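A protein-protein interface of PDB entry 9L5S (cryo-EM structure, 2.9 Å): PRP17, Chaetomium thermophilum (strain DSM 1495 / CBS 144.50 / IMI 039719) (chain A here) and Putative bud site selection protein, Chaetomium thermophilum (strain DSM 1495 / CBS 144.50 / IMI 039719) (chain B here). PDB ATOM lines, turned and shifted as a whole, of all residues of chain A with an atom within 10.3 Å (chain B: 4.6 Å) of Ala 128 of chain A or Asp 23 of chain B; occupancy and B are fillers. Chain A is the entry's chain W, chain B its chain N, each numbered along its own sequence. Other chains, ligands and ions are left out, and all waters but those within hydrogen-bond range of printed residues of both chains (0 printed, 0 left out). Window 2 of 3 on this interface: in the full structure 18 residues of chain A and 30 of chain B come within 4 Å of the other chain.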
ATOM      1  N   GLY A 123       7.973  28.401  25.425  1.00  0.00           N
ATOM      2  CA  GLY A 123       9.259  28.260  26.077  1.00  0.00           C
ATOM      3  C   GLY A 123      10.370  27.998  25.083  1.00  0.00           C
ATOM      4  O   GLY A 123      10.157  27.828  23.877  1.00  0.00           O
ATOM      5  N   SER A 124      11.587  27.969  25.614  1.00  0.00           N
ATOM      6  CA  SER A 124      12.778  27.701  24.826  1.00  0.00           C
ATOM      7  C   SER A 124      13.225  26.270  25.082  1.00  0.00           C
ATOM      8  O   SER A 124      13.376  25.864  26.240  1.00  0.00           O
ATOM      9  CB  SER A 124      13.893  28.685  25.182  1.00  0.00           C
ATOM     10  OG  SER A 124      14.913  28.690  24.200  1.00  0.00           O
ATOM     11  N   ALA A 125      13.429  25.509  24.003  1.00  0.00           N
ATOM     12  CA  ALA A 125      13.836  24.120  24.153  1.00  0.00           C
ATOM     13  C   ALA A 125      15.285  23.973  24.578  1.00  0.00           C
ATOM     14  O   ALA A 125      15.651  22.925  25.114  1.00  0.00           O
ATOM     15  CB  ALA A 125      13.604  23.351  22.853  1.00  0.00           C
ATOM     16  N   THR A 126      16.112  24.991  24.371  1.00  0.00           N
ATOM     17  CA  THR A 126      17.495  24.950  24.818  1.00  0.00           C
ATOM     18  C   THR A 126      17.648  25.412  26.257  1.00  0.00           C
ATOM     19  O   THR A 126      18.771  25.440  26.771  1.00  0.00           O
ATOM     20  CB  THR A 126      18.376  25.805  23.906  1.00  0.00           C
ATOM     21  OG1 THR A 126      17.784  27.100  23.750  1.00  0.00           O
ATOM     22  CG2 THR A 126      18.524  25.142  22.541  1.00  0.00           C
ATOM     23  N   ILE A 127      16.553  25.774  26.916  1.00  0.00           N
ATOM     24  CA  ILE A 127      16.532  26.034  28.349  1.00  0.00           C
ATOM     25  C   ILE A 127      15.916  24.818  29.022  1.00  0.00           C
ATOM     26  O   ILE A 127      14.732  24.520  28.825  1.00  0.00           O
ATOM     27  CB  ILE A 127      15.750  27.315  28.679  1.00  0.00           C
ATOM     28  CG1 ILE A 127      16.500  28.547  28.167  1.00  0.00           C
ATOM     29  CG2 ILE A 127      15.513  27.428  30.171  1.00  0.00           C
ATOM     30  CD1 ILE A 127      15.776  29.855  28.417  1.00  0.00           C
ATOM     31  N   ALA A 128      16.719  24.101  29.807  1.00  0.00           N
ATOM     32  CA  ALA A 128      16.289  22.836  30.386  1.00  0.00           C
ATOM     33  C   ALA A 128      15.656  22.977  31.764  1.00  0.00           C
ATOM     34  O   ALA A 128      15.076  22.005  32.259  1.00  0.00           O
ATOM     35  CB  ALA A 128      17.475  21.871  30.475  1.00  0.00           C
ATOM     36  N   ASP A 129      15.745  24.147  32.393  1.00  0.00           N
ATOM     37  CA  ASP A 129      15.279  24.295  33.765  1.00  0.00           C
ATOM     38  C   ASP A 129      14.900  25.743  34.032  1.00  0.00           C
ATOM     39  O   ASP A 129      15.503  26.664  33.475  1.00  0.00           O
ATOM     40  CB  ASP A 129      16.350  23.842  34.764  1.00  0.00           C
ATOM     41  CG  ASP A 129      15.756  23.225  36.013  1.00  0.00           C
ATOM     42  OD1 ASP A 129      14.619  22.716  35.939  1.00  0.00           O
ATOM     43  OD2 ASP A 129      16.424  23.255  37.069  1.00  0.00           O
ATOM     44  N   GLY A 130      13.900  25.932  34.886  1.00  0.00           N
ATOM     45  CA  GLY A 130      13.539  27.255  35.355  1.00  0.00           C
ATOM     46  C   GLY A 130      12.528  27.949  34.462  1.00  0.00           C
ATOM     47  O   GLY A 130      11.796  27.330  33.684  1.00  0.00           O
ATOM     48  N   GLU A 131      12.482  29.271  34.603  1.00  0.00           N
ATOM     49  CA  GLU A 131      11.626  30.088  33.756  1.00  0.00           C
ATOM     50  C   GLU A 131      12.166  30.087  32.331  1.00  0.00           C
ATOM     51  O   GLU A 131      13.375  30.185  32.107  1.00  0.00           O
ATOM     52  CB  GLU A 131      11.539  31.514  34.310  1.00  0.00           C
ATOM     53  CG  GLU A 131      10.488  32.421  33.657  1.00  0.00           C
ATOM     54  CD  GLU A 131      10.962  33.084  32.376  1.00  0.00           C
ATOM     55  OE1 GLU A 131      12.181  33.318  32.243  1.00  0.00           O
ATOM     56  OE2 GLU A 131      10.116  33.367  31.502  1.00  0.00           O
ATOM     57  N   GLY A 132      11.259  29.978  31.366  1.00  0.00           N
ATOM     58  CA  GLY A 132      11.641  29.859  29.977  1.00  0.00           C
ATOM     59  C   GLY A 132      11.890  28.444  29.508  1.00  0.00           C
ATOM     60  O   GLY A 132      12.238  28.252  28.336  1.00  0.00           O
ATOM     61  N   ALA A 133      11.739  27.453  30.384  1.00  0.00           N
ATOM     62  CA  ALA A 133      11.897  26.062  29.989  1.00  0.00           C
ATOM     63  C   ALA A 133      10.781  25.645  29.039  1.00  0.00           C
ATOM     64  O   ALA A 133       9.677  26.194  29.063  1.00  0.00           O
ATOM     65  CB  ALA A 133      11.909  25.151  31.215  1.00  0.00           C
ATOM     66  N   TYR A 134      11.089  24.669  28.192  1.00  0.00           N
ATOM     67  CA  TYR A 134      10.181  24.272  27.125  1.00  0.00           C
ATOM     68  C   TYR A 134       8.972  23.544  27.696  1.00  0.00           C
ATOM     69  O   TYR A 134       9.114  22.532  28.391  1.00  0.00           O
ATOM     70  CB  TYR A 134      10.907  23.381  26.127  1.00  0.00           C
ATOM     71  CG  TYR A 134      10.077  23.005  24.926  1.00  0.00           C
ATOM     72  CD1 TYR A 134       9.653  23.970  24.022  1.00  0.00           C
ATOM     73  CD2 TYR A 134       9.718  21.686  24.695  1.00  0.00           C
ATOM     74  CE1 TYR A 134       8.896  23.629  22.919  1.00  0.00           C
ATOM     75  CE2 TYR A 134       8.961  21.338  23.599  1.00  0.00           C
ATOM     76  CZ  TYR A 134       8.554  22.310  22.713  1.00  0.00           C
ATOM     77  OH  TYR A 134       7.797  21.963  21.620  1.00  0.00           O
ATOM     78  N   ILE A 135       7.784  24.055  27.394  1.00  0.00           N
ATOM     79  CA  ILE A 135       6.539  23.405  27.765  1.00  0.00           C
ATOM     80  C   ILE A 135       5.870  22.764  26.555  1.00  0.00           C
ATOM     81  O   ILE A 135       5.433  21.614  26.619  1.00  0.00           O
ATOM     82  CB  ILE A 135       5.611  24.424  28.464  1.00  0.00           C
ATOM     83  CG1 ILE A 135       6.031  24.591  29.924  1.00  0.00           C
ATOM     84  CG2 ILE A 135       4.168  23.979  28.415  1.00  0.00           C
ATOM     85  CD1 ILE A 135       5.193  25.586  30.696  1.00  0.00           C
ATOM     86  N   ILE B  20      26.850  20.127  27.146  1.00  0.00           N
ATOM     87  CA  ILE B  20      25.421  19.891  27.312  1.00  0.00           C
ATOM     88  C   ILE B  20      25.120  18.812  28.343  1.00  0.00           C
ATOM     89  O   ILE B  20      23.939  18.493  28.572  1.00  0.00           O
ATOM     90  CB  ILE B  20      24.779  19.531  25.958  1.00  0.00           C
ATOM     91  CG1 ILE B  20      25.182  18.113  25.546  1.00  0.00           C
ATOM     92  CG2 ILE B  20      25.192  20.538  24.895  1.00  0.00           C
ATOM     93  CD1 ILE B  20      24.762  17.733  24.146  1.00  0.00           C
ATOM     94  N   GLU B  21      26.155  18.244  28.973  1.00  0.00           N
ATOM     95  CA  GLU B  21      25.972  17.139  29.910  1.00  0.00           C
ATOM     96  C   GLU B  21      25.133  17.536  31.118  1.00  0.00           C
ATOM     97  O   GLU B  21      24.360  16.718  31.626  1.00  0.00           O
ATOM     98  CB  GLU B  21      27.337  16.616  30.361  1.00  0.00           C
ATOM     99  CG  GLU B  21      27.285  15.342  31.185  1.00  0.00           C
ATOM    100  CD  GLU B  21      28.661  14.847  31.580  1.00  0.00           C
ATOM    101  OE1 GLU B  21      29.660  15.490  31.196  1.00  0.00           O
ATOM    102  OE2 GLU B  21      28.745  13.810  32.272  1.00  0.00           O
ATOM    103  N   GLU B  22      25.252  18.783  31.580  1.00  0.00           N
ATOM    104  CA  GLU B  22      24.481  19.207  32.744  1.00  0.00           C
ATOM    105  C   GLU B  22      22.988  19.247  32.441  1.00  0.00           C
ATOM    106  O   GLU B  22      22.173  18.797  33.254  1.00  0.00           O
ATOM    107  CB  GLU B  22      24.973  20.568  33.233  1.00  0.00           C
ATOM    108  CG  GLU B  22      26.401  20.546  33.751  1.00  0.00           C
ATOM    109  CD  GLU B  22      26.576  19.619  34.941  1.00  0.00           C
ATOM    110  OE1 GLU B  22      25.677  19.579  35.807  1.00  0.00           O
ATOM    111  OE2 GLU B  22      27.612  18.925  35.008  1.00  0.00           O
ATOM    112  N   ASP B  23      22.610  19.738  31.258  1.00  0.00           N
ATOM    113  CA  ASP B  23      21.201  19.731  30.878  1.00  0.00           C
ATOM    114  C   ASP B  23      20.705  18.314  30.610  1.00  0.00           C
ATOM    115  O   ASP B  23      19.535  18.001  30.871  1.00  0.00           O
ATOM    116  CB  ASP B  23      20.983  20.612  29.654  1.00  0.00           C
ATOM    117  CG  ASP B  23      21.434  22.039  29.875  1.00  0.00           C
ATOM    118  OD1 ASP B  23      20.906  22.695  30.796  1.00  0.00           O
ATOM    119  OD2 ASP B  23      22.321  22.505  29.129  1.00  0.00           O
ATOM    120  N   LEU B  24      21.575  17.447  30.082  1.00  0.00           N
ATOM    121  CA  LEU B  24      21.181  16.053  29.882  1.00  0.00           C
ATOM    122  C   LEU B  24      20.900  15.353  31.209  1.00  0.00           C
ATOM    123  O   LEU B  24      19.915  14.614  31.332  1.00  0.00           O
ATOM    124  CB  LEU B  24      22.252  15.309  29.090  1.00  0.00           C
ATOM    125  CG  LEU B  24      22.429  15.775  27.645  1.00  0.00           C
ATOM    126  CD1 LEU B  24      23.328  14.819  26.906  1.00  0.00           C
ATOM    127  CD2 LEU B  24      21.087  15.901  26.937  1.00  0.00           C
ATOM    128  N   LEU B  25      21.739  15.587  32.223  1.00  0.00           N
ATOM    129  CA  LEU B  25      21.430  15.061  33.553  1.00  0.00           C
ATOM    130  C   LEU B  25      20.237  15.761  34.194  1.00  0.00           C
ATOM    131  O   LEU B  25      19.554  15.151  35.022  1.00  0.00           O
ATOM    132  CB  LEU B  25      22.647  15.123  34.485  1.00  0.00           C
ATOM    133  CG  LEU B  25      23.805  14.109  34.414  1.00  0.00           C
ATOM    134  CD1 LEU B  25      24.424  13.871  33.045  1.00  0.00           C
ATOM    135  CD2 LEU B  25      24.882  14.505  35.420  1.00  0.00           C
ATOM    136  N   ILE B  26      19.957  17.016  33.827  1.00  0.00           N
ATOM    137  CA  ILE B  26      18.730  17.665  34.292  1.00  0.00           C
ATOM    138  C   ILE B  26      17.506  16.920  33.769  1.00  0.00           C
ATOM    139  O   ILE B  26      16.573  16.615  34.523  1.00  0.00           O
ATOM    140  CB  ILE B  26      18.713  19.150  33.880  1.00  0.00           C
ATOM    141  CG1 ILE B  26      19.588  19.977  34.821  1.00  0.00           C
ATOM    142  CG2 ILE B  26      17.295  19.707  33.869  1.00  0.00           C
ATOM    143  CD1 ILE B  26      19.727  21.423  34.406  1.00  0.00           C
ATOM    144  N   PHE B  27      17.511  16.587  32.474  1.00  0.00           N
ATOM    145  CA  PHE B  27      16.414  15.812  31.895  1.00  0.00           C
ATOM    146  C   PHE B  27      16.332  14.410  32.494  1.00  0.00           C
ATOM    147  O   PHE B  27      15.233  13.901  32.750  1.00  0.00           O
ATOM    148  CB  PHE B  27      16.563  15.732  30.376  1.00  0.00           C
ATOM    149  CG  PHE B  27      16.296  17.030  29.671  1.00  0.00           C
ATOM    150  CD1 PHE B  27      15.133  17.738  29.920  1.00  0.00           C
ATOM    151  CD2 PHE B  27      17.198  17.534  28.751  1.00  0.00           C
ATOM    152  CE1 PHE B  27      14.879  18.929  29.271  1.00  0.00           C
ATOM    153  CE2 PHE B  27      16.949  18.725  28.099  1.00  0.00           C
ATOM    154  CZ  PHE B  27      15.787  19.422  28.359  1.00  0.00           C
ATOM    155  N   LYS B  30      14.871  14.714  35.906  1.00  0.00           N
ATOM    156  CA  LYS B  30      13.449  15.012  35.766  1.00  0.00           C
ATOM    157  C   LYS B  30      12.650  13.752  35.461  1.00  0.00           C
ATOM    158  O   LYS B  30      11.565  13.545  36.016  1.00  0.00           O
ATOM    159  CB  LYS B  30      13.242  16.056  34.669  1.00  0.00           C
ATOM    160  CG  LYS B  30      11.993  16.899  34.835  1.00  0.00           C
ATOM    161  CD  LYS B  30      11.920  17.974  33.765  1.00  0.00           C
ATOM    162  CE  LYS B  30      12.984  19.036  33.975  1.00  0.00           C
ATOM    163  NZ  LYS B  30      12.589  20.337  33.371  1.00  0.00           N
ATOM    164  N   TYR B  61      15.209  19.555  22.913  1.00  0.00           N
ATOM    165  CA  TYR B  61      16.469  20.209  23.252  1.00  0.00           C
ATOM    166  C   TYR B  61      17.579  19.766  22.308  1.00  0.00           C
ATOM    167  O   TYR B  61      18.308  20.601  21.758  1.00  0.00           O
ATOM    168  CB  TYR B  61      16.808  19.935  24.728  1.00  0.00           C
ATOM    169  CG  TYR B  61      18.186  20.370  25.214  1.00  0.00           C
ATOM    170  CD1 TYR B  61      18.325  21.481  26.035  1.00  0.00           C
ATOM    171  CD2 TYR B  61      19.318  19.587  24.991  1.00  0.00           C
ATOM    172  CE1 TYR B  61      19.563  21.875  26.505  1.00  0.00           C
ATOM    173  CE2 TYR B  61      20.553  19.965  25.464  1.00  0.00           C
ATOM    174  CZ  TYR B  61      20.672  21.107  26.219  1.00  0.00           C
ATOM    175  OH  TYR B  61      21.908  21.477  26.693  1.00  0.00           O
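Of the 10 printed residues of chain B, 5 touch a printed residue of chain A. Of the 13 printed residues of chain A, 3 touch a printed residue of chain B. Among the printed residues, no Asp or Glu carboxylate lies within 4 Å of a Lys or Arg side-chain nitrogen of the other chain.
O of Ala 125 of chain A touches CD1 of Tyr 61 of chain B (3.2 Å). CE1 of Tyr 61 of chain B touches O of Thr 126 of chain A, at 3.7 Å. CB of Ala 128 of chain A touches OD1 of Asp 23 of chain B, at 3.5 Å. CG2 of Ile 26 of chain B touches O of Ala 128 of chain A, 3.6 Å away. CZ of Phe 27 of chain B touches CB of Ala 128 of chain A (3.7 Å).
The side-chain amino group (NZ) of Lys 30 of chain B is in hydrogen-bond range of the backbone carbonyl oxygen (O) of Ala 128 of chain A (3.2 Å).
The side-chain hydroxyl (OG) of Ser 124 of chain A sits at hydrogen-bond distance from the side-chain hydroxyl (OG1) of Thr 126 of chain A, 3.3 Å away. OD2 of Asp 23 of chain B lies within hydrogen-bond range of OH of Tyr 61 of chain B (2.7 Å).
Of the printed residues of chain B, Ala 125 of chain A touches Tyr 61. Of chain B, only Asp 23, Ile 26, Phe 27 and Lys 30 come within 4 Å of Ala 128 of chain A. Ala 133 of chain A touches none of the printed residues of chain B. Asp 23 of chain B touches just one residue of chain A: Ala 128. No residue of chain A comes within 4 Å of Leu 24 of chain B. Of chain A, only Ala 128 comes within 4 Å of Ile 26 of chain B. Phe 27 of chain B touches just one residue of chain A: Ala 128. Of the printed residues of chain A, Lys 30 of chain B touches Ala 128. Of the printed residues of chain A, Tyr 61 of chain B touches Ala 125 and Thr 126.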
